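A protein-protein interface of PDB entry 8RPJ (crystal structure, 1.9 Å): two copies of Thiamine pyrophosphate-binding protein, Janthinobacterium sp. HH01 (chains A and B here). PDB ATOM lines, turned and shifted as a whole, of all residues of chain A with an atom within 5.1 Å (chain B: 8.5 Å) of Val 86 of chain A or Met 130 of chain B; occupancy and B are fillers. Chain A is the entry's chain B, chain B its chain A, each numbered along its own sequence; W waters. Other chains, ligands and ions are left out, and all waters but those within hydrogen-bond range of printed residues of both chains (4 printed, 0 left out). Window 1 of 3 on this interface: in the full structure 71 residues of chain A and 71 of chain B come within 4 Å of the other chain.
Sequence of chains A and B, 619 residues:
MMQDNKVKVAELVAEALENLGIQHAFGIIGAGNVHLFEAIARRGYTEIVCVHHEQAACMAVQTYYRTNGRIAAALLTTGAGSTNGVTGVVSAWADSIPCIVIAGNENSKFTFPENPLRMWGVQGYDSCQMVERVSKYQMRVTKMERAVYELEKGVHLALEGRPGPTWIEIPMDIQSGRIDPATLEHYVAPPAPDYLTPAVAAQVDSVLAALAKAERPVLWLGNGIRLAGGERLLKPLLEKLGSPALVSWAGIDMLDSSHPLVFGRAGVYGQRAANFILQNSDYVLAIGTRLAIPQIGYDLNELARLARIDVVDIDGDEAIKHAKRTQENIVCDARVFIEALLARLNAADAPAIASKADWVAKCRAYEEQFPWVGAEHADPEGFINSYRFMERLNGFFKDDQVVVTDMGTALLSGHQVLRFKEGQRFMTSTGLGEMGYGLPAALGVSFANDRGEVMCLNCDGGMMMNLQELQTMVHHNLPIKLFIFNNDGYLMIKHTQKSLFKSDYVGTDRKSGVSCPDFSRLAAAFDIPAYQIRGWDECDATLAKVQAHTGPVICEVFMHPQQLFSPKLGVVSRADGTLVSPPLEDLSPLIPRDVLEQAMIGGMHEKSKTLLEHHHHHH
The side-chain hydroxyl of Thr 83 of chain A sits at hydrogen-bond distance from the side-chain hydroxyl of Thr 87 of chain B, at 2.7 Å.
The side-chain hydroxyl (OG1) of Thr 87 of chain B sits at hydrogen-bond distance from the side-chain amide oxygen (OD1) of Asn 84 of chain A, at 2.6 Å.
The side-chain amide nitrogen of Gln 129 of chain B is in hydrogen-bond range of the backbone carbonyl oxygen of Gln 129 of chain A, 3.2 Å away.
OG1 of Thr 87 of chain A lies within hydrogen-bond range of OG1 of Thr 83 of chain B, at 2.7 Å.
OD1 of Asn 84 of chain B lies within hydrogen-bond range of OG1 of Thr 87 of chain A.
The side-chain hydroxyl (OH) of Tyr 125 of chain A lies within hydrogen-bond range of the side-chain sulfur (SD) of Met 130 of chain A (3.7 Å).
The backbone carbonyl oxygen (O) of Ala 80 of chain B sits close to the side-chain hydroxyl (OG1) of Thr 83 of chain B, 3.5 Å away.
Val 86 of chain A touches Met 130 of chain B.
Val 90 of chain A touches Thr 83 of chain B.
Arg 133 of chain B touches Gln 129 of chain A (CG to CD, 3.4 Å).
Val 86 of chain B touches Met 130 of chain A (CG1 to CE, 3.5 Å).
Val 134 of chain A touches Met 130 of chain B (CG2 to CE, 3.9 Å).
Of the printed residues of chain B, Asn 84 of chain A touches Thr 87.
No residue of chain B comes within 4 Å of Gly 85 of chain A.
Of the printed residues of chain B, Gln 129 of chain A touches Gln 129 (3.2 Å) and Arg 133 (3.4 Å).
Printed residues of chain A within 4 Å of Thr 87 of chain B: Thr 83 (2.7 Å) and Asn 84 (2.6 Å).
The nearest residue of chain A that does not touch Met 130 of chain B is Val 90 of chain A (4.1 Å).
The nearest printed residue of chain B that does not touch Val 90 of chain A is Met 130 of chain B (4.1 Å).
Of the 14 printed residues of chain A, 8 touch a printed residue of chain B.
Hydrophobic or aromatic side chains of chain A that line the printed part of chain B: Val 86, Val 90, Met 130 and Val 134.
Printed residues of chain B that touch a printed residue of chain A: Ala 80, Thr 83, Asn 84, Val 86, Thr 87, Val 90, Gln 129, Met 130, Arg 133 and Val 134.
Among the printed residues, 14 pairs touch across the chains.
Gln 129 of chain A touches its own counterpart, Gln 129 of chain B.
Met 130 of chain B touches its own counterpart, Met 130 of chain A.
Positions printed for both chains: 82, 83, 84, 85, 86, 87, 89, 90, 125, 129, 130, 131 and 134.
Water W3 lies within hydrogen-bond range of the side-chain amide nitrogen (NE2) of Gln 129 of chain B (2.8 Å) and the side-chain amide nitrogen (NE2) of Gln 129 of chain A (3.0 Å).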
ATOM      1  N   SER A  82       8.731  16.690 -24.918  1.00  0.00           N
ATOM      2  CA  SER A  82       7.497  16.534 -25.682  1.00  0.00           C
ATOM      3  C   SER A  82       6.364  17.396 -25.139  1.00  0.00           C
ATOM      4  O   SER A  82       5.662  18.052 -25.918  1.00  0.00           O
ATOM      5  CB  SER A  82       7.093  15.061 -25.710  1.00  0.00           C
ATOM      6  OG  SER A  82       8.037  14.313 -26.454  1.00  0.00           O
ATOM      7  N   THR A  83       6.172  17.424 -23.816  1.00  0.00           N
ATOM      8  CA  THR A  83       5.102  18.244 -23.257  1.00  0.00           C
ATOM      9  C   THR A  83       5.337  19.724 -23.554  1.00  0.00           C
ATOM     10  O   THR A  83       4.377  20.483 -23.719  1.00  0.00           O
ATOM     11  CB  THR A  83       4.969  18.014 -21.749  1.00  0.00           C
ATOM     12  OG1 THR A  83       6.176  18.403 -21.078  1.00  0.00           O
ATOM     13  CG2 THR A  83       4.667  16.546 -21.432  1.00  0.00           C
ATOM     14  N   ASN A  84       6.599  20.142 -23.656  1.00  0.00           N
ATOM     15  CA  ASN A  84       6.894  21.539 -23.954  1.00  0.00           C
ATOM     16  C   ASN A  84       6.504  21.938 -25.369  1.00  0.00           C
ATOM     17  O   ASN A  84       6.374  23.137 -25.647  1.00  0.00           O
ATOM     18  CB  ASN A  84       8.383  21.826 -23.758  1.00  0.00           C
ATOM     19  CG  ASN A  84       8.732  22.223 -22.338  1.00  0.00           C
ATOM     20  OD1 ASN A  84       7.874  22.288 -21.458  1.00  0.00           O
ATOM     21  ND2 ASN A  84      10.013  22.485 -22.104  1.00  0.00           N
ATOM     22  N   GLY A  85       6.328  20.981 -26.274  1.00  0.00           N
ATOM     23  CA  GLY A  85       5.942  21.338 -27.626  1.00  0.00           C
ATOM     24  C   GLY A  85       4.458  21.514 -27.863  1.00  0.00           C
ATOM     25  O   GLY A  85       4.076  21.983 -28.940  1.00  0.00           O
ATOM     26  N   VAL A  86       3.611  21.183 -26.891  1.00  0.00           N
ATOM     27  CA  VAL A  86       2.194  20.990 -27.195  1.00  0.00           C
ATOM     28  C   VAL A  86       1.542  22.286 -27.670  1.00  0.00           C
ATOM     29  O   VAL A  86       0.707  22.270 -28.581  1.00  0.00           O
ATOM     30  CB  VAL A  86       1.472  20.393 -25.974  1.00  0.00           C
ATOM     31  CG1 VAL A  86      -0.026  20.439 -26.155  1.00  0.00           C
ATOM     32  CG2 VAL A  86       1.908  18.955 -25.769  1.00  0.00           C
ATOM     33  N   THR A  87       1.919  23.427 -27.090  1.00  0.00           N
ATOM     34  CA  THR A  87       1.289  24.679 -27.494  1.00  0.00           C
ATOM     35  C   THR A  87       1.499  24.948 -28.979  1.00  0.00           C
ATOM     36  O   THR A  87       0.579  25.395 -29.672  1.00  0.00           O
ATOM     37  CB  THR A  87       1.835  25.834 -26.658  1.00  0.00           C
ATOM     38  OG1 THR A  87       1.466  25.621 -25.290  1.00  0.00           O
ATOM     39  CG2 THR A  87       1.266  27.162 -27.139  1.00  0.00           C
ATOM     40  N   GLY A  88       2.710  24.693 -29.480  1.00  0.00           N
ATOM     41  CA  GLY A  88       2.972  24.882 -30.892  1.00  0.00           C
ATOM     42  C   GLY A  88       2.196  23.921 -31.771  1.00  0.00           C
ATOM     43  O   GLY A  88       1.786  24.277 -32.879  1.00  0.00           O
ATOM     44  N   VAL A  89       1.986  22.693 -31.301  1.00  0.00           N
ATOM     45  CA  VAL A  89       1.160  21.762 -32.057  1.00  0.00           C
ATOM     46  C   VAL A  89      -0.254  22.308 -32.182  1.00  0.00           C
ATOM     47  O   VAL A  89      -0.848  22.291 -33.265  1.00  0.00           O
ATOM     48  CB  VAL A  89       1.191  20.366 -31.404  1.00  0.00           C
ATOM     49  CG1 VAL A  89       0.191  19.440 -32.079  1.00  0.00           C
ATOM     50  CG2 VAL A  89       2.610  19.807 -31.465  1.00  0.00           C
ATOM     51  N   VAL A  90      -0.806  22.832 -31.086  1.00  0.00           N
ATOM     52  CA  VAL A  90      -2.183  23.309 -31.122  1.00  0.00           C
ATOM     53  C   VAL A  90      -2.320  24.506 -32.060  1.00  0.00           C
ATOM     54  O   VAL A  90      -3.321  24.629 -32.777  1.00  0.00           O
ATOM     55  CB  VAL A  90      -2.688  23.637 -29.703  1.00  0.00           C
ATOM     56  CG1 VAL A  90      -4.117  24.164 -29.766  1.00  0.00           C
ATOM     57  CG2 VAL A  90      -2.633  22.402 -28.827  1.00  0.00           C
ATOM     58  N   TYR A 125       5.989   9.263 -21.166  1.00  0.00           N
ATOM     59  CA  TYR A 125       4.529   9.200 -21.084  1.00  0.00           C
ATOM     60  C   TYR A 125       4.001   8.988 -22.501  1.00  0.00           C
ATOM     61  O   TYR A 125       4.764   8.965 -23.471  1.00  0.00           O
ATOM     62  CB  TYR A 125       3.959  10.469 -20.423  1.00  0.00           C
ATOM     63  CG  TYR A 125       4.021  11.651 -21.355  1.00  0.00           C
ATOM     64  CD1 TYR A 125       5.221  12.303 -21.589  1.00  0.00           C
ATOM     65  CD2 TYR A 125       2.892  12.089 -22.037  1.00  0.00           C
ATOM     66  CE1 TYR A 125       5.293  13.368 -22.471  1.00  0.00           C
ATOM     67  CE2 TYR A 125       2.953  13.147 -22.912  1.00  0.00           C
ATOM     68  CZ  TYR A 125       4.160  13.785 -23.130  1.00  0.00           C
ATOM     69  OH  TYR A 125       4.209  14.846 -24.009  1.00  0.00           O
ATOM     70  N   GLN A 129      -1.167  10.198 -27.129  1.00  0.00           N
ATOM     71  CA  GLN A 129      -2.490  10.441 -26.561  1.00  0.00           C
ATOM     72  C   GLN A 129      -2.674  11.909 -26.228  1.00  0.00           C
ATOM     73  O   GLN A 129      -3.771  12.460 -26.378  1.00  0.00           O
ATOM     74  CB  GLN A 129      -2.683   9.579 -25.316  1.00  0.00           C
ATOM     75  CG  GLN A 129      -3.987   9.825 -24.553  1.00  0.00           C
ATOM     76  CD  GLN A 129      -3.961  11.053 -23.649  1.00  0.00           C
ATOM     77  OE1 GLN A 129      -2.900  11.511 -23.218  1.00  0.00           O
ATOM     78  NE2 GLN A 129      -5.139  11.591 -23.360  1.00  0.00           N
ATOM     79  N   MET A 130      -1.605  12.562 -25.768  1.00  0.00           N
ATOM     80  CA  MET A 130      -1.731  13.937 -25.314  1.00  0.00           C
ATOM     81  C   MET A 130      -2.103  14.884 -26.447  1.00  0.00           C
ATOM     82  O   MET A 130      -2.762  15.898 -26.199  1.00  0.00           O
ATOM     83  CB  MET A 130      -0.429  14.376 -24.641  1.00  0.00           C
ATOM     84  CG  MET A 130      -0.447  15.814 -24.159  1.00  0.00           C
ATOM     85  SD  MET A 130       0.944  16.253 -23.095  1.00  0.00           S
ATOM     86  CE  MET A 130       0.448  15.472 -21.564  1.00  0.00           C
ATOM     87  N   VAL A 131      -1.717  14.577 -27.690  1.00  0.00           N
ATOM     88  CA  VAL A 131      -2.029  15.426 -28.837  1.00  0.00           C
ATOM     89  C   VAL A 131      -3.073  14.790 -29.746  1.00  0.00           C
ATOM     90  O   VAL A 131      -3.304  15.276 -30.859  1.00  0.00           O
ATOM     91  CB  VAL A 131      -0.759  15.778 -29.634  1.00  0.00           C
ATOM     92  CG1 VAL A 131       0.161  16.618 -28.776  1.00  0.00           C
ATOM     93  CG2 VAL A 131      -0.058  14.516 -30.132  1.00  0.00           C
ATOM     94  N   VAL A 134      -5.604  17.266 -31.193  1.00  0.00           N
ATOM     95  CA  VAL A 134      -5.094  18.522 -31.727  1.00  0.00           C
ATOM     96  C   VAL A 134      -4.010  18.244 -32.762  1.00  0.00           C
ATOM     97  O   VAL A 134      -3.098  19.057 -32.961  1.00  0.00           O
ATOM     98  CB  VAL A 134      -4.579  19.426 -30.593  1.00  0.00           C
ATOM     99  CG1 VAL A 134      -5.750  19.856 -29.720  1.00  0.00           C
ATOM    100  CG2 VAL A 134      -3.533  18.709 -29.748  1.00  0.00           C
ATOM    101  N   GLY B  79      -7.126  28.203 -24.160  1.00  0.00           N
ATOM    102  CA  GLY B  79      -6.190  28.065 -25.265  1.00  0.00           C
ATOM    103  C   GLY B  79      -4.783  27.844 -24.763  1.00  0.00           C
ATOM    104  O   GLY B  79      -4.521  26.935 -23.963  1.00  0.00           O
ATOM    105  N   ALA B  80      -3.850  28.675 -25.243  1.00  0.00           N
ATOM    106  CA  ALA B  80      -2.444  28.535 -24.874  1.00  0.00           C
ATOM    107  C   ALA B  80      -2.227  28.774 -23.389  1.00  0.00           C
ATOM    108  O   ALA B  80      -1.237  28.293 -22.832  1.00  0.00           O
ATOM    109  CB  ALA B  80      -1.595  29.499 -25.706  1.00  0.00           C
ATOM    110  N   SER B  82      -3.793  27.261 -21.208  1.00  0.00           N
ATOM    111  CA  SER B  82      -3.900  25.912 -20.664  1.00  0.00           C
ATOM    112  C   SER B  82      -2.814  24.983 -21.206  1.00  0.00           C
ATOM    113  O   SER B  82      -2.213  24.221 -20.449  1.00  0.00           O
ATOM    114  CB  SER B  82      -5.284  25.342 -20.964  1.00  0.00           C
ATOM    115  OG  SER B  82      -6.292  26.015 -20.238  1.00  0.00           O
ATOM    116  N   THR B  83      -2.567  25.019 -22.522  1.00  0.00           N
ATOM    117  CA  THR B  83      -1.538  24.140 -23.057  1.00  0.00           C
ATOM    118  C   THR B  83      -0.172  24.471 -22.464  1.00  0.00           C
ATOM    119  O   THR B  83       0.645  23.569 -22.247  1.00  0.00           O
ATOM    120  CB  THR B  83      -1.488  24.219 -24.578  1.00  0.00           C
ATOM    121  OG1 THR B  83      -1.259  25.566 -25.000  1.00  0.00           O
ATOM    122  CG2 THR B  83      -2.790  23.729 -25.181  1.00  0.00           C
ATOM    123  N   ASN B  84       0.081  25.751 -22.172  1.00  0.00           N
ATOM    124  CA  ASN B  84       1.361  26.128 -21.588  1.00  0.00           C
ATOM    125  C   ASN B  84       1.562  25.553 -20.189  1.00  0.00           C
ATOM    126  O   ASN B  84       2.696  25.551 -19.691  1.00  0.00           O
ATOM    127  CB  ASN B  84       1.502  27.652 -21.504  1.00  0.00           C
ATOM    128  CG  ASN B  84       2.048  28.263 -22.781  1.00  0.00           C
ATOM    129  OD1 ASN B  84       2.459  27.558 -23.702  1.00  0.00           O
ATOM    130  ND2 ASN B  84       2.064  29.589 -22.832  1.00  0.00           N
ATOM    131  N   GLY B  85       0.501  25.085 -19.530  1.00  0.00           N
ATOM    132  CA  GLY B  85       0.659  24.521 -18.201  1.00  0.00           C
ATOM    133  C   GLY B  85       1.009  23.050 -18.126  1.00  0.00           C
ATOM    134  O   GLY B  85       1.372  22.566 -17.050  1.00  0.00           O
ATOM    135  N   VAL B  86       0.952  22.324 -19.239  1.00  0.00           N
ATOM    136  CA  VAL B  86       0.918  20.863 -19.157  1.00  0.00           C
ATOM    137  C   VAL B  86       2.216  20.303 -18.580  1.00  0.00           C
ATOM    138  O   VAL B  86       2.193  19.314 -17.835  1.00  0.00           O
ATOM    139  CB  VAL B  86       0.587  20.259 -20.537  1.00  0.00           C
ATOM    140  CG1 VAL B  86       0.761  18.744 -20.510  1.00  0.00           C
ATOM    141  CG2 VAL B  86      -0.838  20.638 -20.943  1.00  0.00           C
ATOM    142  N   THR B  87       3.365  20.902 -18.905  1.00  0.00           N
ATOM    143  CA  THR B  87       4.621  20.355 -18.396  1.00  0.00           C
ATOM    144  C   THR B  87       4.633  20.336 -16.872  1.00  0.00           C
ATOM    145  O   THR B  87       5.089  19.366 -16.252  1.00  0.00           O
ATOM    146  CB  THR B  87       5.804  21.160 -18.919  1.00  0.00           C
ATOM    147  OG1 THR B  87       5.878  21.032 -20.340  1.00  0.00           O
ATOM    148  CG2 THR B  87       7.113  20.673 -18.301  1.00  0.00           C
ATOM    149  N   VAL B  89       1.997  20.111 -14.960  1.00  0.00           N
ATOM    150  CA  VAL B  89       1.064  19.086 -14.495  1.00  0.00           C
ATOM    151  C   VAL B  89       1.744  17.721 -14.486  1.00  0.00           C
ATOM    152  O   VAL B  89       1.610  16.951 -13.525  1.00  0.00           O
ATOM    153  CB  VAL B  89      -0.215  19.075 -15.359  1.00  0.00           C
ATOM    154  CG1 VAL B  89      -1.140  17.899 -14.981  1.00  0.00           C
ATOM    155  CG2 VAL B  89      -0.967  20.402 -15.225  1.00  0.00           C
ATOM    156  N   VAL B  90       2.498  17.405 -15.540  1.00  0.00           N
ATOM    157  CA  VAL B  90       3.146  16.101 -15.617  1.00  0.00           C
ATOM    158  C   VAL B  90       4.197  15.957 -14.520  1.00  0.00           C
ATOM    159  O   VAL B  90       4.361  14.875 -13.939  1.00  0.00           O
ATOM    160  CB  VAL B  90       3.753  15.874 -17.012  1.00  0.00           C
ATOM    161  CG1 VAL B  90       4.435  14.514 -17.081  1.00  0.00           C
ATOM    162  CG2 VAL B  90       2.682  15.984 -18.072  1.00  0.00           C
ATOM    163  N   TYR B 125     -10.090  24.430 -26.564  1.00  0.00           N
ATOM    164  CA  TYR B 125      -9.929  23.011 -26.870  1.00  0.00           C
ATOM    165  C   TYR B 125     -10.275  22.223 -25.602  1.00  0.00           C
ATOM    166  O   TYR B 125     -10.552  22.804 -24.545  1.00  0.00           O
ATOM    167  CB  TYR B 125      -8.503  22.718 -27.365  1.00  0.00           C
ATOM    168  CG  TYR B 125      -7.511  22.757 -26.235  1.00  0.00           C
ATOM    169  CD1 TYR B 125      -7.116  23.965 -25.679  1.00  0.00           C
ATOM    170  CD2 TYR B 125      -7.017  21.586 -25.679  1.00  0.00           C
ATOM    171  CE1 TYR B 125      -6.242  24.010 -24.615  1.00  0.00           C
ATOM    172  CE2 TYR B 125      -6.138  21.618 -24.619  1.00  0.00           C
ATOM    173  CZ  TYR B 125      -5.754  22.833 -24.088  1.00  0.00           C
ATOM    174  OH  TYR B 125      -4.878  22.871 -23.029  1.00  0.00           O
ATOM    175  N   ASP B 126     -10.256  20.894 -25.705  1.00  0.00           N
ATOM    176  CA  ASP B 126     -10.600  20.036 -24.563  1.00  0.00           C
ATOM    177  C   ASP B 126      -9.385  19.917 -23.650  1.00  0.00           C
ATOM    178  O   ASP B 126      -8.582  18.986 -23.753  1.00  0.00           O
ATOM    179  CB  ASP B 126     -11.083  18.666 -25.022  1.00  0.00           C
ATOM    180  CG  ASP B 126     -11.658  17.836 -23.880  1.00  0.00           C
ATOM    181  OD1 ASP B 126     -11.432  18.200 -22.708  1.00  0.00           O
ATOM    182  OD2 ASP B 126     -12.343  16.828 -24.154  1.00  0.00           O
ATOM    183  N   SER B 127      -9.266  20.871 -22.727  1.00  0.00           N
ATOM    184  CA  SER B 127      -8.124  20.913 -21.820  1.00  0.00           C
ATOM    185  C   SER B 127      -8.133  19.753 -20.831  1.00  0.00           C
ATOM    186  O   SER B 127      -7.064  19.368 -20.342  1.00  0.00           O
ATOM    187  CB  SER B 127      -8.104  22.254 -21.087  1.00  0.00           C
ATOM    188  OG  SER B 127      -9.022  22.279 -20.011  1.00  0.00           O
ATOM    189  N   CYS B 128      -9.305  19.171 -20.552  1.00  0.00           N
ATOM    190  CA  CYS B 128      -9.368  18.009 -19.670  1.00  0.00           C
ATOM    191  C   CYS B 128      -8.785  16.769 -20.345  1.00  0.00           C
ATOM    192  O   CYS B 128      -8.006  16.025 -19.736  1.00  0.00           O
ATOM    193  CB  CYS B 128     -10.814  17.753 -19.245  1.00  0.00           C
ATOM    194  SG  CYS B 128     -11.532  19.017 -18.166  1.00  0.00           S
ATOM    195  N   GLN B 129      -9.168  16.515 -21.605  1.00  0.00           N
ATOM    196  CA  GLN B 129      -8.658  15.338 -22.312  1.00  0.00           C
ATOM    197  C   GLN B 129      -7.138  15.367 -22.403  1.00  0.00           C
ATOM    198  O   GLN B 129      -6.478  14.327 -22.300  1.00  0.00           O
ATOM    199  CB  GLN B 129      -9.266  15.258 -23.712  1.00  0.00           C
ATOM    200  CG  GLN B 129      -8.760  14.096 -24.583  1.00  0.00           C
ATOM    201  CD  GLN B 129      -7.413  14.360 -25.262  1.00  0.00           C
ATOM    202  OE1 GLN B 129      -6.997  15.505 -25.440  1.00  0.00           O
ATOM    203  NE2 GLN B 129      -6.731  13.282 -25.642  1.00  0.00           N
ATOM    204  N   MET B 130      -6.561  16.554 -22.602  1.00  0.00           N
ATOM    205  CA  MET B 130      -5.123  16.638 -22.823  1.00  0.00           C
ATOM    206  C   MET B 130      -4.326  16.166 -21.612  1.00  0.00           C
ATOM    207  O   MET B 130      -3.212  15.653 -21.775  1.00  0.00           O
ATOM    208  CB  MET B 130      -4.751  18.076 -23.203  1.00  0.00           C
ATOM    209  CG  MET B 130      -3.272  18.287 -23.455  1.00  0.00           C
ATOM    210  SD  MET B 130      -2.889  19.855 -24.272  1.00  0.00           S
ATOM    211  CE  MET B 130      -3.435  19.528 -25.944  1.00  0.00           C
ATOM    212  N   VAL B 131      -4.867  16.313 -20.399  1.00  0.00           N
ATOM    213  CA  VAL B 131      -4.169  15.911 -19.177  1.00  0.00           C
ATOM    214  C   VAL B 131      -4.772  14.652 -18.558  1.00  0.00           C
ATOM    215  O   VAL B 131      -4.406  14.276 -17.437  1.00  0.00           O
ATOM    216  CB  VAL B 131      -4.124  17.057 -18.150  1.00  0.00           C
ATOM    217  CG1 VAL B 131      -3.268  18.204 -18.680  1.00  0.00           C
ATOM    218  CG2 VAL B 131      -5.518  17.554 -17.764  1.00  0.00           C
ATOM    219  N   GLU B 132      -5.650  13.969 -19.284  1.00  0.00           N
ATOM    220  CA  GLU B 132      -6.388  12.821 -18.768  1.00  0.00           C
ATOM    221  C   GLU B 132      -5.497  11.694 -18.268  1.00  0.00           C
ATOM    222  O   GLU B 132      -5.898  10.955 -17.360  1.00  0.00           O
ATOM    223  CB  GLU B 132      -7.269  12.309 -19.891  1.00  0.00           C
ATOM    224  CG  GLU B 132      -8.511  11.567 -19.533  1.00  0.00           C
ATOM    225  CD  GLU B 132      -9.372  11.417 -20.760  1.00  0.00           C
ATOM    226  OE1 GLU B 132      -8.956  10.710 -21.706  1.00  0.00           O
ATOM    227  OE2 GLU B 132     -10.443  12.053 -20.808  1.00  0.00           O
ATOM    228  N   ARG B 133      -4.323  11.507 -18.859  1.00  0.00           N
ATOM    229  CA  ARG B 133      -3.453  10.403 -18.479  1.00  0.00           C
ATOM    230  C   ARG B 133      -2.355  10.823 -17.514  1.00  0.00           C
ATOM    231  O   ARG B 133      -1.559   9.975 -17.089  1.00  0.00           O
ATOM    232  CB  ARG B 133      -2.811   9.767 -19.718  1.00  0.00           C
ATOM    233  CG  ARG B 133      -3.790   9.260 -20.764  1.00  0.00           C
ATOM    234  CD  ARG B 133      -4.627   8.106 -20.245  1.00  0.00           C
ATOM    235  NE  ARG B 133      -3.805   7.011 -19.741  1.00  0.00           N
ATOM    236  CZ  ARG B 133      -4.284   5.943 -19.120  1.00  0.00           C
ATOM    237  NH1 ARG B 133      -5.581   5.782 -18.929  1.00  0.00           N
ATOM    238  NH2 ARG B 133      -3.440   5.018 -18.676  1.00  0.00           N
ATOM    239  N   VAL B 134      -2.300  12.106 -17.155  1.00  0.00           N
ATOM    240  CA  VAL B 134      -1.226  12.645 -16.338  1.00  0.00           C
ATOM    241  C   VAL B 134      -1.793  13.501 -15.212  1.00  0.00           C
ATOM    242  O   VAL B 134      -1.146  14.451 -14.754  1.00  0.00           O
ATOM    243  CB  VAL B 134      -0.244  13.459 -17.199  1.00  0.00           C
ATOM    244  CG1 VAL B 134       0.498  12.554 -18.170  1.00  0.00           C
ATOM    245  CG2 VAL B 134      -0.977  14.551 -17.987  1.00  0.00           C
ATOM    246  N   SER B 135      -3.004  13.183 -14.763  1.00  0.00           N
ATOM    247  CA  SER B 135      -3.615  13.866 -13.626  1.00  0.00           C
ATOM    248  C   SER B 135      -4.587  12.901 -12.961  1.00  0.00           C
ATOM    249  O   SER B 135      -5.032  11.921 -13.566  1.00  0.00           O
ATOM    250  CB  SER B 135      -4.313  15.169 -14.044  1.00  0.00           C
ATOM    251  OG  SER B 135      -5.371  14.955 -14.956  1.00  0.00           O
ATOM    252  N   GLN B 138     -10.063  15.095 -13.681  1.00  0.00           N
ATOM    253  CA  GLN B 138     -10.354  16.221 -14.556  1.00  0.00           C
ATOM    254  C   GLN B 138     -11.868  16.360 -14.589  1.00  0.00           C
ATOM    255  O   GLN B 138     -12.579  15.354 -14.678  1.00  0.00           O
ATOM    256  CB  GLN B 138      -9.834  16.030 -15.989  1.00  0.00           C
ATOM    257  CG  GLN B 138      -8.491  15.343 -16.138  1.00  0.00           C
ATOM    258  CD  GLN B 138      -8.598  13.847 -15.967  1.00  0.00           C
ATOM    259  OE1 GLN B 138      -9.548  13.218 -16.442  1.00  0.00           O
ATOM    260  NE2 GLN B 138      -7.630  13.264 -15.275  1.00  0.00           N
ATOM    261  N   ARG B 140     -14.950  19.217 -16.280  1.00  0.00           N
ATOM    262  CA  ARG B 140     -15.467  20.456 -16.846  1.00  0.00           C
ATOM    263  C   ARG B 140     -16.788  20.773 -16.155  1.00  0.00           C
ATOM    264  O   ARG B 140     -17.717  19.956 -16.181  1.00  0.00           O
ATOM    265  CB  ARG B 140     -15.665  20.333 -18.355  1.00  0.00           C
ATOM    266  CG  ARG B 140     -16.225  21.597 -19.009  1.00  0.00           C
ATOM    267  CD  ARG B 140     -16.266  21.484 -20.537  1.00  0.00           C
ATOM    268  NE  ARG B 140     -14.927  21.247 -21.057  1.00  0.00           N
ATOM    269  CZ  ARG B 140     -14.466  20.064 -21.438  1.00  0.00           C
ATOM    270  NH1 ARG B 140     -15.264  19.020 -21.575  1.00  0.00           N
ATOM    271  NH2 ARG B 140     -13.169  19.922 -21.676  1.00  0.00           N
ATOM    272  N   TRP B 167      -7.477  18.802 -12.323  1.00  0.00           N
ATOM    273  CA  TRP B 167      -7.703  19.778 -13.387  1.00  0.00           C
ATOM    274  C   TRP B 167      -9.196  20.066 -13.472  1.00  0.00           C
ATOM    275  O   TRP B 167      -9.972  19.208 -13.895  1.00  0.00           O
ATOM    276  CB  TRP B 167      -7.165  19.263 -14.730  1.00  0.00           C
ATOM    277  CG  TRP B 167      -7.212  20.281 -15.835  1.00  0.00           C
ATOM    278  CD1 TRP B 167      -8.325  20.708 -16.507  1.00  0.00           C
ATOM    279  CD2 TRP B 167      -6.105  21.001 -16.398  1.00  0.00           C
ATOM    280  NE1 TRP B 167      -7.978  21.651 -17.448  1.00  0.00           N
ATOM    281  CE2 TRP B 167      -6.625  21.849 -17.403  1.00  0.00           C
ATOM    282  CE3 TRP B 167      -4.728  21.014 -16.156  1.00  0.00           C
ATOM    283  CZ2 TRP B 167      -5.813  22.698 -18.156  1.00  0.00           C
ATOM    284  CZ3 TRP B 167      -3.927  21.859 -16.908  1.00  0.00           C
ATOM    285  CH2 TRP B 167      -4.472  22.689 -17.894  1.00  0.00           C
ATOM    286  N   GLU B 169     -11.927  22.578 -15.149  1.00  0.00           N
ATOM    287  CA  GLU B 169     -12.157  23.542 -16.214  1.00  0.00           C
ATOM    288  C   GLU B 169     -13.497  24.217 -15.965  1.00  0.00           C
ATOM    289  O   GLU B 169     -14.505  23.535 -15.741  1.00  0.00           O
ATOM    290  CB  GLU B 169     -12.148  22.836 -17.556  1.00  0.00           C
ATOM    291  CG  GLU B 169     -12.074  23.763 -18.740  1.00  0.00           C
ATOM    292  CD  GLU B 169     -12.487  23.079 -20.022  1.00  0.00           C
ATOM    293  OE1 GLU B 169     -11.767  22.165 -20.479  1.00  0.00           O
ATOM    294  OE2 GLU B 169     -13.539  23.461 -20.574  1.00  0.00           O
HETATM  295  O   HOH W   1      -2.972  12.977 -20.902  1.00  0.00           O
HETATM  296  O   HOH W   2      -5.213  15.966 -27.463  1.00  0.00           O
HETATM  297  O   HOH W   3      -7.515  10.651 -24.923  1.00  0.00           O
HETATM  298  O   HOH W   4       3.278  22.955 -22.813  1.00  0.00           O
